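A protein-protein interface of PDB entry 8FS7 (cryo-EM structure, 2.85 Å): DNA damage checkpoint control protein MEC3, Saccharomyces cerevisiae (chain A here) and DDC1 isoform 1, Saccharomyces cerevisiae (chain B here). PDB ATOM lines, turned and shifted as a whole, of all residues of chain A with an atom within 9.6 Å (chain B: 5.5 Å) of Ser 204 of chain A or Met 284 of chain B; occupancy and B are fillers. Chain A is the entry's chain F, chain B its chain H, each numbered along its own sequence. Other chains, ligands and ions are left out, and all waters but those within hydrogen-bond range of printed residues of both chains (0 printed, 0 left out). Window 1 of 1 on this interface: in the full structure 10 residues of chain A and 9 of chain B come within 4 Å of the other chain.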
ATOM      1  N   SER A  99       4.766   6.995  -1.049  1.00  0.00           N
ATOM      2  CA  SER A  99       3.514   7.382  -0.403  1.00  0.00           C
ATOM      3  C   SER A  99       2.335   7.216  -1.354  1.00  0.00           C
ATOM      4  O   SER A  99       1.282   6.684  -0.972  1.00  0.00           O
ATOM      5  CB  SER A  99       3.608   8.824   0.099  1.00  0.00           C
ATOM      6  OG  SER A  99       4.727   8.996   0.950  1.00  0.00           O
ATOM      7  N   SER A 102       1.674   3.518  -1.756  1.00  0.00           N
ATOM      8  CA  SER A 102       0.962   2.970  -0.606  1.00  0.00           C
ATOM      9  C   SER A 102      -0.511   3.362  -0.634  1.00  0.00           C
ATOM     10  O   SER A 102      -1.387   2.539  -0.336  1.00  0.00           O
ATOM     11  CB  SER A 102       1.619   3.443   0.691  1.00  0.00           C
ATOM     12  OG  SER A 102       3.009   3.176   0.684  1.00  0.00           O
ATOM     13  N   VAL A 103      -0.799   4.615  -0.997  1.00  0.00           N
ATOM     14  CA  VAL A 103      -2.185   5.062  -1.112  1.00  0.00           C
ATOM     15  C   VAL A 103      -2.919   4.250  -2.173  1.00  0.00           C
ATOM     16  O   VAL A 103      -4.062   3.819  -1.970  1.00  0.00           O
ATOM     17  CB  VAL A 103      -2.226   6.573  -1.417  1.00  0.00           C
ATOM     18  CG1 VAL A 103      -3.483   6.942  -2.196  1.00  0.00           C
ATOM     19  CG2 VAL A 103      -2.130   7.374  -0.132  1.00  0.00           C
ATOM     20  N   ARG A 106      -3.637   0.733  -0.891  1.00  0.00           N
ATOM     21  CA  ARG A 106      -4.788   0.762   0.010  1.00  0.00           C
ATOM     22  C   ARG A 106      -6.089   0.870  -0.774  1.00  0.00           C
ATOM     23  O   ARG A 106      -7.055   0.143  -0.506  1.00  0.00           O
ATOM     24  CB  ARG A 106      -4.657   1.923   0.997  1.00  0.00           C
ATOM     25  CG  ARG A 106      -3.485   1.807   1.958  1.00  0.00           C
ATOM     26  CD  ARG A 106      -3.960   1.637   3.393  1.00  0.00           C
ATOM     27  NE  ARG A 106      -5.032   0.656   3.509  1.00  0.00           N
ATOM     28  CZ  ARG A 106      -5.877   0.591   4.529  1.00  0.00           C
ATOM     29  NH1 ARG A 106      -5.801   1.435   5.545  1.00  0.00           N
ATOM     30  NH2 ARG A 106      -6.822  -0.345   4.530  1.00  0.00           N
ATOM     31  N   ARG A 109      -6.887  -2.402  -2.476  1.00  0.00           N
ATOM     32  CA  ARG A 109      -7.426  -3.380  -1.537  1.00  0.00           C
ATOM     33  C   ARG A 109      -8.826  -2.999  -1.076  1.00  0.00           C
ATOM     34  O   ARG A 109      -9.570  -3.859  -0.589  1.00  0.00           O
ATOM     35  CB  ARG A 109      -6.501  -3.535  -0.331  1.00  0.00           C
ATOM     36  CG  ARG A 109      -6.320  -4.979   0.117  1.00  0.00           C
ATOM     37  CD  ARG A 109      -5.092  -5.183   1.002  1.00  0.00           C
ATOM     38  NE  ARG A 109      -5.208  -4.510   2.292  1.00  0.00           N
ATOM     39  CZ  ARG A 109      -4.760  -3.289   2.555  1.00  0.00           C
ATOM     40  NH1 ARG A 109      -4.107  -2.580   1.649  1.00  0.00           N
ATOM     41  NH2 ARG A 109      -4.967  -2.770   3.761  1.00  0.00           N
ATOM     42  N   VAL A 110      -9.197  -1.723  -1.205  1.00  0.00           N
ATOM     43  CA  VAL A 110     -10.543  -1.296  -0.830  1.00  0.00           C
ATOM     44  C   VAL A 110     -11.584  -1.958  -1.730  1.00  0.00           C
ATOM     45  O   VAL A 110     -12.604  -2.471  -1.253  1.00  0.00           O
ATOM     46  CB  VAL A 110     -10.645   0.241  -0.861  1.00  0.00           C
ATOM     47  CG1 VAL A 110     -12.085   0.687  -0.939  1.00  0.00           C
ATOM     48  CG2 VAL A 110      -9.997   0.836   0.378  1.00  0.00           C
ATOM     49  N   MET A 119     -12.161   7.824  -5.385  1.00  0.00           N
ATOM     50  CA  MET A 119     -10.990   8.384  -4.717  1.00  0.00           C
ATOM     51  C   MET A 119     -10.894   9.865  -5.065  1.00  0.00           C
ATOM     52  O   MET A 119     -10.596  10.222  -6.208  1.00  0.00           O
ATOM     53  CB  MET A 119      -9.720   7.642  -5.128  1.00  0.00           C
ATOM     54  CG  MET A 119      -8.436   8.304  -4.661  1.00  0.00           C
ATOM     55  SD  MET A 119      -7.034   7.935  -5.732  1.00  0.00           S
ATOM     56  CE  MET A 119      -6.289   6.570  -4.847  1.00  0.00           C
ATOM     57  N   THR A 120     -11.139  10.723  -4.078  1.00  0.00           N
ATOM     58  CA  THR A 120     -11.100  12.165  -4.280  1.00  0.00           C
ATOM     59  C   THR A 120      -9.719  12.701  -3.928  1.00  0.00           C
ATOM     60  O   THR A 120      -9.203  12.439  -2.837  1.00  0.00           O
ATOM     61  CB  THR A 120     -12.166  12.859  -3.430  1.00  0.00           C
ATOM     62  OG1 THR A 120     -13.430  12.210  -3.621  1.00  0.00           O
ATOM     63  CG2 THR A 120     -12.290  14.323  -3.823  1.00  0.00           C
ATOM     64  N   GLN A 124      -4.373  20.588  -1.468  1.00  0.00           N
ATOM     65  CA  GLN A 124      -4.569  21.406  -0.278  1.00  0.00           C
ATOM     66  C   GLN A 124      -3.213  21.875   0.237  1.00  0.00           C
ATOM     67  O   GLN A 124      -2.356  21.053   0.576  1.00  0.00           O
ATOM     68  CB  GLN A 124      -5.314  20.623   0.802  1.00  0.00           C
ATOM     69  CG  GLN A 124      -6.439  19.751   0.269  1.00  0.00           C
ATOM     70  CD  GLN A 124      -6.967  18.781   1.307  1.00  0.00           C
ATOM     71  OE1 GLN A 124      -6.516  18.773   2.452  1.00  0.00           O
ATOM     72  NE2 GLN A 124      -7.929  17.956   0.911  1.00  0.00           N
ATOM     73  N   LEU A 156      -1.312  16.655  -1.386  1.00  0.00           N
ATOM     74  CA  LEU A 156      -2.569  16.237  -1.992  1.00  0.00           C
ATOM     75  C   LEU A 156      -3.436  15.538  -0.953  1.00  0.00           C
ATOM     76  O   LEU A 156      -2.974  14.624  -0.261  1.00  0.00           O
ATOM     77  CB  LEU A 156      -2.332  15.306  -3.184  1.00  0.00           C
ATOM     78  CG  LEU A 156      -1.424  15.787  -4.316  1.00  0.00           C
ATOM     79  CD1 LEU A 156      -0.236  14.856  -4.462  1.00  0.00           C
ATOM     80  CD2 LEU A 156      -2.189  15.895  -5.625  1.00  0.00           C
ATOM     81  N   GLY A 157      -4.690  15.970  -0.848  1.00  0.00           N
ATOM     82  CA  GLY A 157      -5.629  15.359   0.070  1.00  0.00           C
ATOM     83  C   GLY A 157      -6.355  14.176  -0.536  1.00  0.00           C
ATOM     84  O   GLY A 157      -7.544  14.266  -0.856  1.00  0.00           O
ATOM     85  N   ILE A 158      -5.648  13.062  -0.700  1.00  0.00           N
ATOM     86  CA  ILE A 158      -6.219  11.864  -1.308  1.00  0.00           C
ATOM     87  C   ILE A 158      -7.069  11.153  -0.261  1.00  0.00           C
ATOM     88  O   ILE A 158      -6.544  10.453   0.607  1.00  0.00           O
ATOM     89  CB  ILE A 158      -5.127  10.938  -1.856  1.00  0.00           C
ATOM     90  CG1 ILE A 158      -4.114  11.739  -2.677  1.00  0.00           C
ATOM     91  CG2 ILE A 158      -5.741   9.830  -2.692  1.00  0.00           C
ATOM     92  CD1 ILE A 158      -2.701  11.213  -2.579  1.00  0.00           C
ATOM     93  N   THR A 159      -8.387  11.333  -0.341  1.00  0.00           N
ATOM     94  CA  THR A 159      -9.322  10.723   0.594  1.00  0.00           C
ATOM     95  C   THR A 159     -10.326   9.868  -0.163  1.00  0.00           C
ATOM     96  O   THR A 159     -10.834  10.273  -1.214  1.00  0.00           O
ATOM     97  CB  THR A 159     -10.074  11.779   1.421  1.00  0.00           C
ATOM     98  OG1 THR A 159     -11.228  12.226   0.698  1.00  0.00           O
ATOM     99  CG2 THR A 159      -9.179  12.972   1.730  1.00  0.00           C
ATOM    100  N   PHE A 160     -10.610   8.684   0.376  1.00  0.00           N
ATOM    101  CA  PHE A 160     -11.618   7.795  -0.186  1.00  0.00           C
ATOM    102  C   PHE A 160     -12.304   7.060   0.959  1.00  0.00           C
ATOM    103  O   PHE A 160     -11.914   7.177   2.123  1.00  0.00           O
ATOM    104  CB  PHE A 160     -11.005   6.823  -1.202  1.00  0.00           C
ATOM    105  CG  PHE A 160      -9.784   6.102  -0.703  1.00  0.00           C
ATOM    106  CD1 PHE A 160      -9.903   4.899  -0.025  1.00  0.00           C
ATOM    107  CD2 PHE A 160      -8.518   6.616  -0.927  1.00  0.00           C
ATOM    108  CE1 PHE A 160      -8.783   4.230   0.431  1.00  0.00           C
ATOM    109  CE2 PHE A 160      -7.394   5.952  -0.473  1.00  0.00           C
ATOM    110  CZ  PHE A 160      -7.527   4.757   0.205  1.00  0.00           C
ATOM    111  N   GLU A 161     -13.335   6.294   0.617  1.00  0.00           N
ATOM    112  CA  GLU A 161     -14.142   5.577   1.592  1.00  0.00           C
ATOM    113  C   GLU A 161     -13.991   4.071   1.413  1.00  0.00           C
ATOM    114  O   GLU A 161     -13.548   3.584   0.369  1.00  0.00           O
ATOM    115  CB  GLU A 161     -15.620   5.969   1.473  1.00  0.00           C
ATOM    116  CG  GLU A 161     -15.922   7.405   1.867  1.00  0.00           C
ATOM    117  CD  GLU A 161     -16.819   7.496   3.085  1.00  0.00           C
ATOM    118  OE1 GLU A 161     -17.444   6.475   3.441  1.00  0.00           O
ATOM    119  OE2 GLU A 161     -16.903   8.589   3.683  1.00  0.00           O
ATOM    120  N   GLU A 162     -14.371   3.338   2.457  1.00  0.00           N
ATOM    121  CA  GLU A 162     -14.335   1.883   2.444  1.00  0.00           C
ATOM    122  C   GLU A 162     -15.429   1.368   3.368  1.00  0.00           C
ATOM    123  O   GLU A 162     -15.685   1.957   4.422  1.00  0.00           O
ATOM    124  CB  GLU A 162     -12.960   1.356   2.875  1.00  0.00           C
ATOM    125  CG  GLU A 162     -12.744  -0.133   2.639  1.00  0.00           C
ATOM    126  CD  GLU A 162     -13.216  -0.987   3.798  1.00  0.00           C
ATOM    127  OE1 GLU A 162     -13.442  -0.429   4.892  1.00  0.00           O
ATOM    128  OE2 GLU A 162     -13.362  -2.214   3.613  1.00  0.00           O
ATOM    129  N   ILE A 201     -15.767   3.926   7.004  1.00  0.00           N
ATOM    130  CA  ILE A 201     -14.381   4.086   7.433  1.00  0.00           C
ATOM    131  C   ILE A 201     -13.720   5.027   6.434  1.00  0.00           C
ATOM    132  O   ILE A 201     -13.427   4.635   5.300  1.00  0.00           O
ATOM    133  CB  ILE A 201     -13.633   2.749   7.517  1.00  0.00           C
ATOM    134  CG1 ILE A 201     -14.285   1.837   8.557  1.00  0.00           C
ATOM    135  CG2 ILE A 201     -12.167   2.974   7.848  1.00  0.00           C
ATOM    136  CD1 ILE A 201     -14.462   0.413   8.094  1.00  0.00           C
ATOM    137  N   MET A 202     -13.488   6.269   6.849  1.00  0.00           N
ATOM    138  CA  MET A 202     -12.902   7.266   5.961  1.00  0.00           C
ATOM    139  C   MET A 202     -11.383   7.148   5.976  1.00  0.00           C
ATOM    140  O   MET A 202     -10.755   7.237   7.036  1.00  0.00           O
ATOM    141  CB  MET A 202     -13.337   8.667   6.385  1.00  0.00           C
ATOM    142  CG  MET A 202     -14.210   9.381   5.368  1.00  0.00           C
ATOM    143  SD  MET A 202     -13.340   9.750   3.833  1.00  0.00           S
ATOM    144  CE  MET A 202     -12.325  11.132   4.347  1.00  0.00           C
ATOM    145  N   HIS A 203     -10.793   6.947   4.800  1.00  0.00           N
ATOM    146  CA  HIS A 203      -9.343   6.861   4.659  1.00  0.00           C
ATOM    147  C   HIS A 203      -8.828   8.204   4.152  1.00  0.00           C
ATOM    148  O   HIS A 203      -9.101   8.590   3.012  1.00  0.00           O
ATOM    149  CB  HIS A 203      -8.960   5.731   3.708  1.00  0.00           C
ATOM    150  CG  HIS A 203      -9.274   4.365   4.232  1.00  0.00           C
ATOM    151  ND1 HIS A 203      -8.411   3.663   5.047  1.00  0.00           N
ATOM    152  CD2 HIS A 203     -10.354   3.568   4.055  1.00  0.00           C
ATOM    153  CE1 HIS A 203      -8.947   2.495   5.350  1.00  0.00           C
ATOM    154  NE2 HIS A 203     -10.127   2.412   4.760  1.00  0.00           N
ATOM    155  N   SER A 204      -8.084   8.912   4.996  1.00  0.00           N
ATOM    156  CA  SER A 204      -7.538  10.220   4.659  1.00  0.00           C
ATOM    157  C   SER A 204      -6.018  10.144   4.584  1.00  0.00           C
ATOM    158  O   SER A 204      -5.375   9.536   5.445  1.00  0.00           O
ATOM    159  CB  SER A 204      -7.958  11.273   5.688  1.00  0.00           C
ATOM    160  OG  SER A 204      -9.362  11.272   5.875  1.00  0.00           O
ATOM    161  N   PHE A 205      -5.452  10.764   3.551  1.00  0.00           N
ATOM    162  CA  PHE A 205      -4.014  10.744   3.332  1.00  0.00           C
ATOM    163  C   PHE A 205      -3.543  12.122   2.891  1.00  0.00           C
ATOM    164  O   PHE A 205      -4.284  12.873   2.251  1.00  0.00           O
ATOM    165  CB  PHE A 205      -3.616   9.698   2.283  1.00  0.00           C
ATOM    166  CG  PHE A 205      -4.019   8.295   2.640  1.00  0.00           C
ATOM    167  CD1 PHE A 205      -3.175   7.488   3.385  1.00  0.00           C
ATOM    168  CD2 PHE A 205      -5.236   7.781   2.225  1.00  0.00           C
ATOM    169  CE1 PHE A 205      -3.541   6.197   3.714  1.00  0.00           C
ATOM    170  CE2 PHE A 205      -5.607   6.491   2.551  1.00  0.00           C
ATOM    171  CZ  PHE A 205      -4.759   5.698   3.296  1.00  0.00           C
ATOM    172  N   LYS A 206      -2.299  12.445   3.242  1.00  0.00           N
ATOM    173  CA  LYS A 206      -1.671  13.707   2.854  1.00  0.00           C
ATOM    174  C   LYS A 206      -0.230  13.411   2.462  1.00  0.00           C
ATOM    175  O   LYS A 206       0.596  13.091   3.324  1.00  0.00           O
ATOM    176  CB  LYS A 206      -1.730  14.733   3.986  1.00  0.00           C
ATOM    177  CG  LYS A 206      -3.134  15.210   4.328  1.00  0.00           C
ATOM    178  CD  LYS A 206      -3.120  16.200   5.482  1.00  0.00           C
ATOM    179  CE  LYS A 206      -4.529  16.639   5.847  1.00  0.00           C
ATOM    180  NZ  LYS A 206      -5.219  17.304   4.708  1.00  0.00           N
ATOM    181  N   VAL A 207       0.070  13.515   1.174  1.00  0.00           N
ATOM    182  CA  VAL A 207       1.394  13.212   0.637  1.00  0.00           C
ATOM    183  C   VAL A 207       2.126  14.529   0.404  1.00  0.00           C
ATOM    184  O   VAL A 207       1.683  15.325  -0.438  1.00  0.00           O
ATOM    185  CB  VAL A 207       1.302  12.398  -0.662  1.00  0.00           C
ATOM    186  CG1 VAL A 207       2.682  12.218  -1.276  1.00  0.00           C
ATOM    187  CG2 VAL A 207       0.644  11.052  -0.400  1.00  0.00           C
ATOM    188  N   PRO A 208       3.225  14.800   1.108  1.00  0.00           N
ATOM    189  CA  PRO A 208       3.937  16.067   0.903  1.00  0.00           C
ATOM    190  C   PRO A 208       4.599  16.120  -0.466  1.00  0.00           C
ATOM    191  O   PRO A 208       5.313  15.199  -0.870  1.00  0.00           O
ATOM    192  CB  PRO A 208       4.980  16.077   2.028  1.00  0.00           C
ATOM    193  CG  PRO A 208       4.521  15.035   3.005  1.00  0.00           C
ATOM    194  CD  PRO A 208       3.822  14.000   2.188  1.00  0.00           C
ATOM    195  N   PHE B 240      -5.764  -0.774  10.185  1.00  0.00           N
ATOM    196  CA  PHE B 240      -5.189   0.559  10.036  1.00  0.00           C
ATOM    197  C   PHE B 240      -3.755   0.609  10.550  1.00  0.00           C
ATOM    198  O   PHE B 240      -2.878   1.207   9.918  1.00  0.00           O
ATOM    199  CB  PHE B 240      -6.053   1.591  10.760  1.00  0.00           C
ATOM    200  CG  PHE B 240      -5.449   2.967  10.793  1.00  0.00           C
ATOM    201  CD1 PHE B 240      -5.335   3.714   9.632  1.00  0.00           C
ATOM    202  CD2 PHE B 240      -4.988   3.509  11.981  1.00  0.00           C
ATOM    203  CE1 PHE B 240      -4.777   4.979   9.656  1.00  0.00           C
ATOM    204  CE2 PHE B 240      -4.428   4.773  12.011  1.00  0.00           C
ATOM    205  CZ  PHE B 240      -4.322   5.508  10.847  1.00  0.00           C
ATOM    206  N   ASN B 243      -1.371  -1.301   8.311  1.00  0.00           N
ATOM    207  CA  ASN B 243      -1.141  -0.574   7.071  1.00  0.00           C
ATOM    208  C   ASN B 243      -0.137   0.561   7.234  1.00  0.00           C
ATOM    209  O   ASN B 243       0.394   1.049   6.230  1.00  0.00           O
ATOM    210  CB  ASN B 243      -2.459  -0.025   6.525  1.00  0.00           C
ATOM    211  CG  ASN B 243      -3.256  -1.071   5.778  1.00  0.00           C
ATOM    212  OD1 ASN B 243      -3.058  -1.281   4.581  1.00  0.00           O
ATOM    213  ND2 ASN B 243      -4.164  -1.737   6.479  1.00  0.00           N
ATOM    214  N   CYS B 244       0.131   0.990   8.464  1.00  0.00           N
ATOM    215  CA  CYS B 244       1.102   2.045   8.706  1.00  0.00           C
ATOM    216  C   CYS B 244       2.524   1.501   8.615  1.00  0.00           C
ATOM    217  O   CYS B 244       2.776   0.304   8.772  1.00  0.00           O
ATOM    218  CB  CYS B 244       0.879   2.685  10.076  1.00  0.00           C
ATOM    219  SG  CYS B 244      -0.715   3.509  10.279  1.00  0.00           S
ATOM    220  N   THR B 249       6.392   6.952   9.610  1.00  0.00           N
ATOM    221  CA  THR B 249       5.439   7.457  10.586  1.00  0.00           C
ATOM    222  C   THR B 249       5.841   6.968  11.971  1.00  0.00           C
ATOM    223  O   THR B 249       6.184   5.795  12.143  1.00  0.00           O
ATOM    224  CB  THR B 249       4.018   7.000  10.249  1.00  0.00           C
ATOM    225  OG1 THR B 249       3.603   7.602   9.016  1.00  0.00           O
ATOM    226  CG2 THR B 249       3.053   7.403  11.344  1.00  0.00           C
ATOM    227  N   ILE B 263      -8.425   8.306  14.416  1.00  0.00           N
ATOM    228  CA  ILE B 263      -7.043   7.981  14.749  1.00  0.00           C
ATOM    229  C   ILE B 263      -6.197   8.228  13.508  1.00  0.00           C
ATOM    230  O   ILE B 263      -6.427   7.615  12.458  1.00  0.00           O
ATOM    231  CB  ILE B 263      -6.895   6.533  15.250  1.00  0.00           C
ATOM    232  CG1 ILE B 263      -5.428   6.096  15.207  1.00  0.00           C
ATOM    233  CG2 ILE B 263      -7.790   5.583  14.457  1.00  0.00           C
ATOM    234  CD1 ILE B 263      -5.183   4.722  15.790  1.00  0.00           C
ATOM    235  N   THR B 264      -5.230   9.135  13.623  1.00  0.00           N
ATOM    236  CA  THR B 264      -4.358   9.500  12.513  1.00  0.00           C
ATOM    237  C   THR B 264      -2.913   9.236  12.907  1.00  0.00           C
ATOM    238  O   THR B 264      -2.481   9.614  14.002  1.00  0.00           O
ATOM    239  CB  THR B 264      -4.554  10.965  12.109  1.00  0.00           C
ATOM    240  OG1 THR B 264      -3.467  11.384  11.273  1.00  0.00           O
ATOM    241  CG2 THR B 264      -4.640  11.866  13.328  1.00  0.00           C
ATOM    242  N   ALA B 265      -2.175   8.578  12.020  1.00  0.00           N
ATOM    243  CA  ALA B 265      -0.757   8.306  12.224  1.00  0.00           C
ATOM    244  C   ALA B 265       0.042   9.296  11.383  1.00  0.00           C
ATOM    245  O   ALA B 265       0.124   9.155  10.159  1.00  0.00           O
ATOM    246  CB  ALA B 265      -0.432   6.863  11.854  1.00  0.00           C
ATOM    247  N   PHE B 266       0.632  10.296  12.035  1.00  0.00           N
ATOM    248  CA  PHE B 266       1.276  11.403  11.343  1.00  0.00           C
ATOM    249  C   PHE B 266       2.732  11.505  11.784  1.00  0.00           C
ATOM    250  O   PHE B 266       3.231  10.691  12.568  1.00  0.00           O
ATOM    251  CB  PHE B 266       0.535  12.724  11.603  1.00  0.00           C
ATOM    252  CG  PHE B 266       0.696  13.251  13.007  1.00  0.00           C
ATOM    253  CD1 PHE B 266      -0.112  12.795  14.032  1.00  0.00           C
ATOM    254  CD2 PHE B 266       1.672  14.193  13.301  1.00  0.00           C
ATOM    255  CE1 PHE B 266       0.046  13.276  15.319  1.00  0.00           C
ATOM    256  CE2 PHE B 266       1.829  14.676  14.584  1.00  0.00           C
ATOM    257  CZ  PHE B 266       1.013  14.217  15.594  1.00  0.00           C
ATOM    258  N   LEU B 282       4.213  13.495   6.749  1.00  0.00           N
ATOM    259  CA  LEU B 282       3.238  12.568   6.192  1.00  0.00           C
ATOM    260  C   LEU B 282       2.166  12.293   7.240  1.00  0.00           C
ATOM    261  O   LEU B 282       2.484  11.940   8.381  1.00  0.00           O
ATOM    262  CB  LEU B 282       3.919  11.266   5.760  1.00  0.00           C
ATOM    263  CG  LEU B 282       3.386  10.455   4.570  1.00  0.00           C
ATOM    264  CD1 LEU B 282       4.215   9.192   4.393  1.00  0.00           C
ATOM    265  CD2 LEU B 282       1.910  10.098   4.702  1.00  0.00           C
ATOM    266  N   SER B 283       0.901  12.454   6.852  1.00  0.00           N
ATOM    267  CA  SER B 283      -0.236  12.298   7.761  1.00  0.00           C
ATOM    268  C   SER B 283      -1.222  11.302   7.154  1.00  0.00           C
ATOM    269  O   SER B 283      -2.034  11.660   6.297  1.00  0.00           O
ATOM    270  CB  SER B 283      -0.898  13.644   8.038  1.00  0.00           C
ATOM    271  OG  SER B 283      -2.048  13.489   8.852  1.00  0.00           O
ATOM    272  N   MET B 284      -1.147  10.051   7.605  1.00  0.00           N
ATOM    273  CA  MET B 284      -2.097   9.016   7.210  1.00  0.00           C
ATOM    274  C   MET B 284      -3.173   8.929   8.287  1.00  0.00           C
ATOM    275  O   MET B 284      -2.889   8.558   9.431  1.00  0.00           O
ATOM    276  CB  MET B 284      -1.382   7.681   7.013  1.00  0.00           C
ATOM    277  CG  MET B 284      -2.277   6.457   7.088  1.00  0.00           C
ATOM    278  SD  MET B 284      -1.331   4.924   7.027  1.00  0.00           S
ATOM    279  CE  MET B 284      -2.649   3.712   6.988  1.00  0.00           C
ATOM    280  N   SER B 285      -4.404   9.277   7.927  1.00  0.00           N
ATOM    281  CA  SER B 285      -5.491   9.440   8.882  1.00  0.00           C
ATOM    282  C   SER B 285      -6.576   8.390   8.654  1.00  0.00           C
ATOM    283  O   SER B 285      -6.579   7.660   7.659  1.00  0.00           O
ATOM    284  CB  SER B 285      -6.072  10.853   8.790  1.00  0.00           C
ATOM    285  OG  SER B 285      -7.195  10.999   9.640  1.00  0.00           O
ATOM    286  N   ASN B 286      -7.510   8.330   9.603  1.00  0.00           N
ATOM    287  CA  ASN B 286      -8.650   7.425   9.551  1.00  0.00           C
ATOM    288  C   ASN B 286      -9.702   7.924  10.531  1.00  0.00           C
ATOM    289  O   ASN B 286      -9.365   8.351  11.638  1.00  0.00           O
ATOM    290  CB  ASN B 286      -8.236   5.986   9.892  1.00  0.00           C
ATOM    291  CG  ASN B 286      -9.294   4.964   9.515  1.00  0.00           C
ATOM    292  OD1 ASN B 286     -10.473   5.289   9.381  1.00  0.00           O
ATOM    293  ND2 ASN B 286      -8.872   3.717   9.340  1.00  0.00           N
ATOM    294  N   THR B 287     -10.969   7.863  10.121  1.00  0.00           N
ATOM    295  CA  THR B 287     -12.076   8.357  10.932  1.00  0.00           C
ATOM    296  C   THR B 287     -13.192   7.322  10.943  1.00  0.00           C
ATOM    297  O   THR B 287     -13.521   6.752   9.899  1.00  0.00           O
ATOM    298  CB  THR B 287     -12.599   9.697  10.396  1.00  0.00           C
ATOM    299  OG1 THR B 287     -11.503  10.605  10.229  1.00  0.00           O
ATOM    300  CG2 THR B 287     -13.605  10.306  11.363  1.00  0.00           C
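The guanidinium group of Arg 109 of chain A lies within hydrogen-bond range of the side-chain amide oxygen of Asn 243 of chain B (2.6 Å).
The backbone carbonyl oxygen (O) of Thr 287 of chain B sits at hydrogen-bond distance from the backbone NH (N) of Met 202 of chain A.
The side-chain amide oxygen (OD1) of Asn 243 of chain B sits at hydrogen-bond distance from the guanidinium group (NE) of Arg 106 of chain A (3.0 Å).
O of Ser 204 of chain A is in hydrogen-bond range of N of Ser 285 of chain B, at 2.7 Å.
O of Met 202 of chain A lies close to OD1 of Asn 286 of chain B, at 3.1 Å.
The backbone NH (N) of Lys 206 of chain A lies within hydrogen-bond range of the backbone carbonyl oxygen (O) of Ser 283 of chain B, 3.2 Å away.
The backbone NH (N) of Phe 205 of chain A is in hydrogen-bond range of the backbone carbonyl oxygen (O) of Ile 158 of chain A (3.2 Å).
The side-chain sulfur of Cys 244 of chain B sits at hydrogen-bond distance from the side-chain sulfur of Met 284 of chain B, at 3.6 Å.
The side-chain hydroxyl (OG1) of Thr 264 of chain B is in hydrogen-bond range of the backbone carbonyl oxygen (O) of Met 284 of chain B, at 3.4 Å.
The backbone carbonyl oxygen of Glu 162 of chain A lies within hydrogen-bond range of the backbone NH of Ile 201 of chain A (3.2 Å).
N of Ile 263 of chain B is in hydrogen-bond range of O of Asn 286 of chain B.
A ring nitrogen (ND1) of His 203 of chain A sits close to the guanidinium group of Arg 106 of chain A (3.5 Å).
Among the printed residues, merely in contact across the chains: Ile 201 of chain A with Asn 286 of chain B, Ser 99 of chain A with Leu 282 of chain B, Lys 206 of chain A with Leu 282 of chain B, Phe 205 of chain A with Met 284 of chain B, Ser 204 of chain A with Met 284 of chain B, Phe 205 of chain A with Ser 283 of chain B and Ile 201 of chain A with Thr 287 of chain B.
Ser 102 of chain A touches none of the printed residues of chain B.
Of the printed residues of chain B, Arg 109 of chain A touches Asn 243 (2.6 Å).
Ile 158 of chain A touches none of the printed residues of chain B.
Printed residues of chain B within 4 Å of Ile 201 of chain A: Asn 286 and Thr 287.
Ser 204 of chain A touches just these residues of chain B: Met 284 and Ser 285.
No residue of chain A comes within 4 Å of Thr 264 of chain B.
No residue of chain A comes within 4 Å of Ala 265 of chain B.
Of the printed residues of chain A, Ser 283 of chain B touches Phe 205 and Lys 206.
Of chain A, only Ser 204 and Phe 205 come within 4 Å of Met 284 of chain B.
Ser 285 of chain B touches just one residue of chain A: Ser 204.
The nearest printed residue of chain A that does not touch Asn 243 of chain B is Ser 102 of chain A (6.2 Å).
Of the 24 printed residues of chain A, 8 touch a printed residue of chain B.
Hydrophobic or aromatic side chains of chain A within 4 Å of the printed part of chain B: Ile 201 and Phe 205.
Of the 14 printed residues of chain B, 7 touch a printed residue of chain A.
Hydrophobic or aromatic side chains of chain B within 4 Å of the printed part of chain A: Leu 282 and Met 284.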
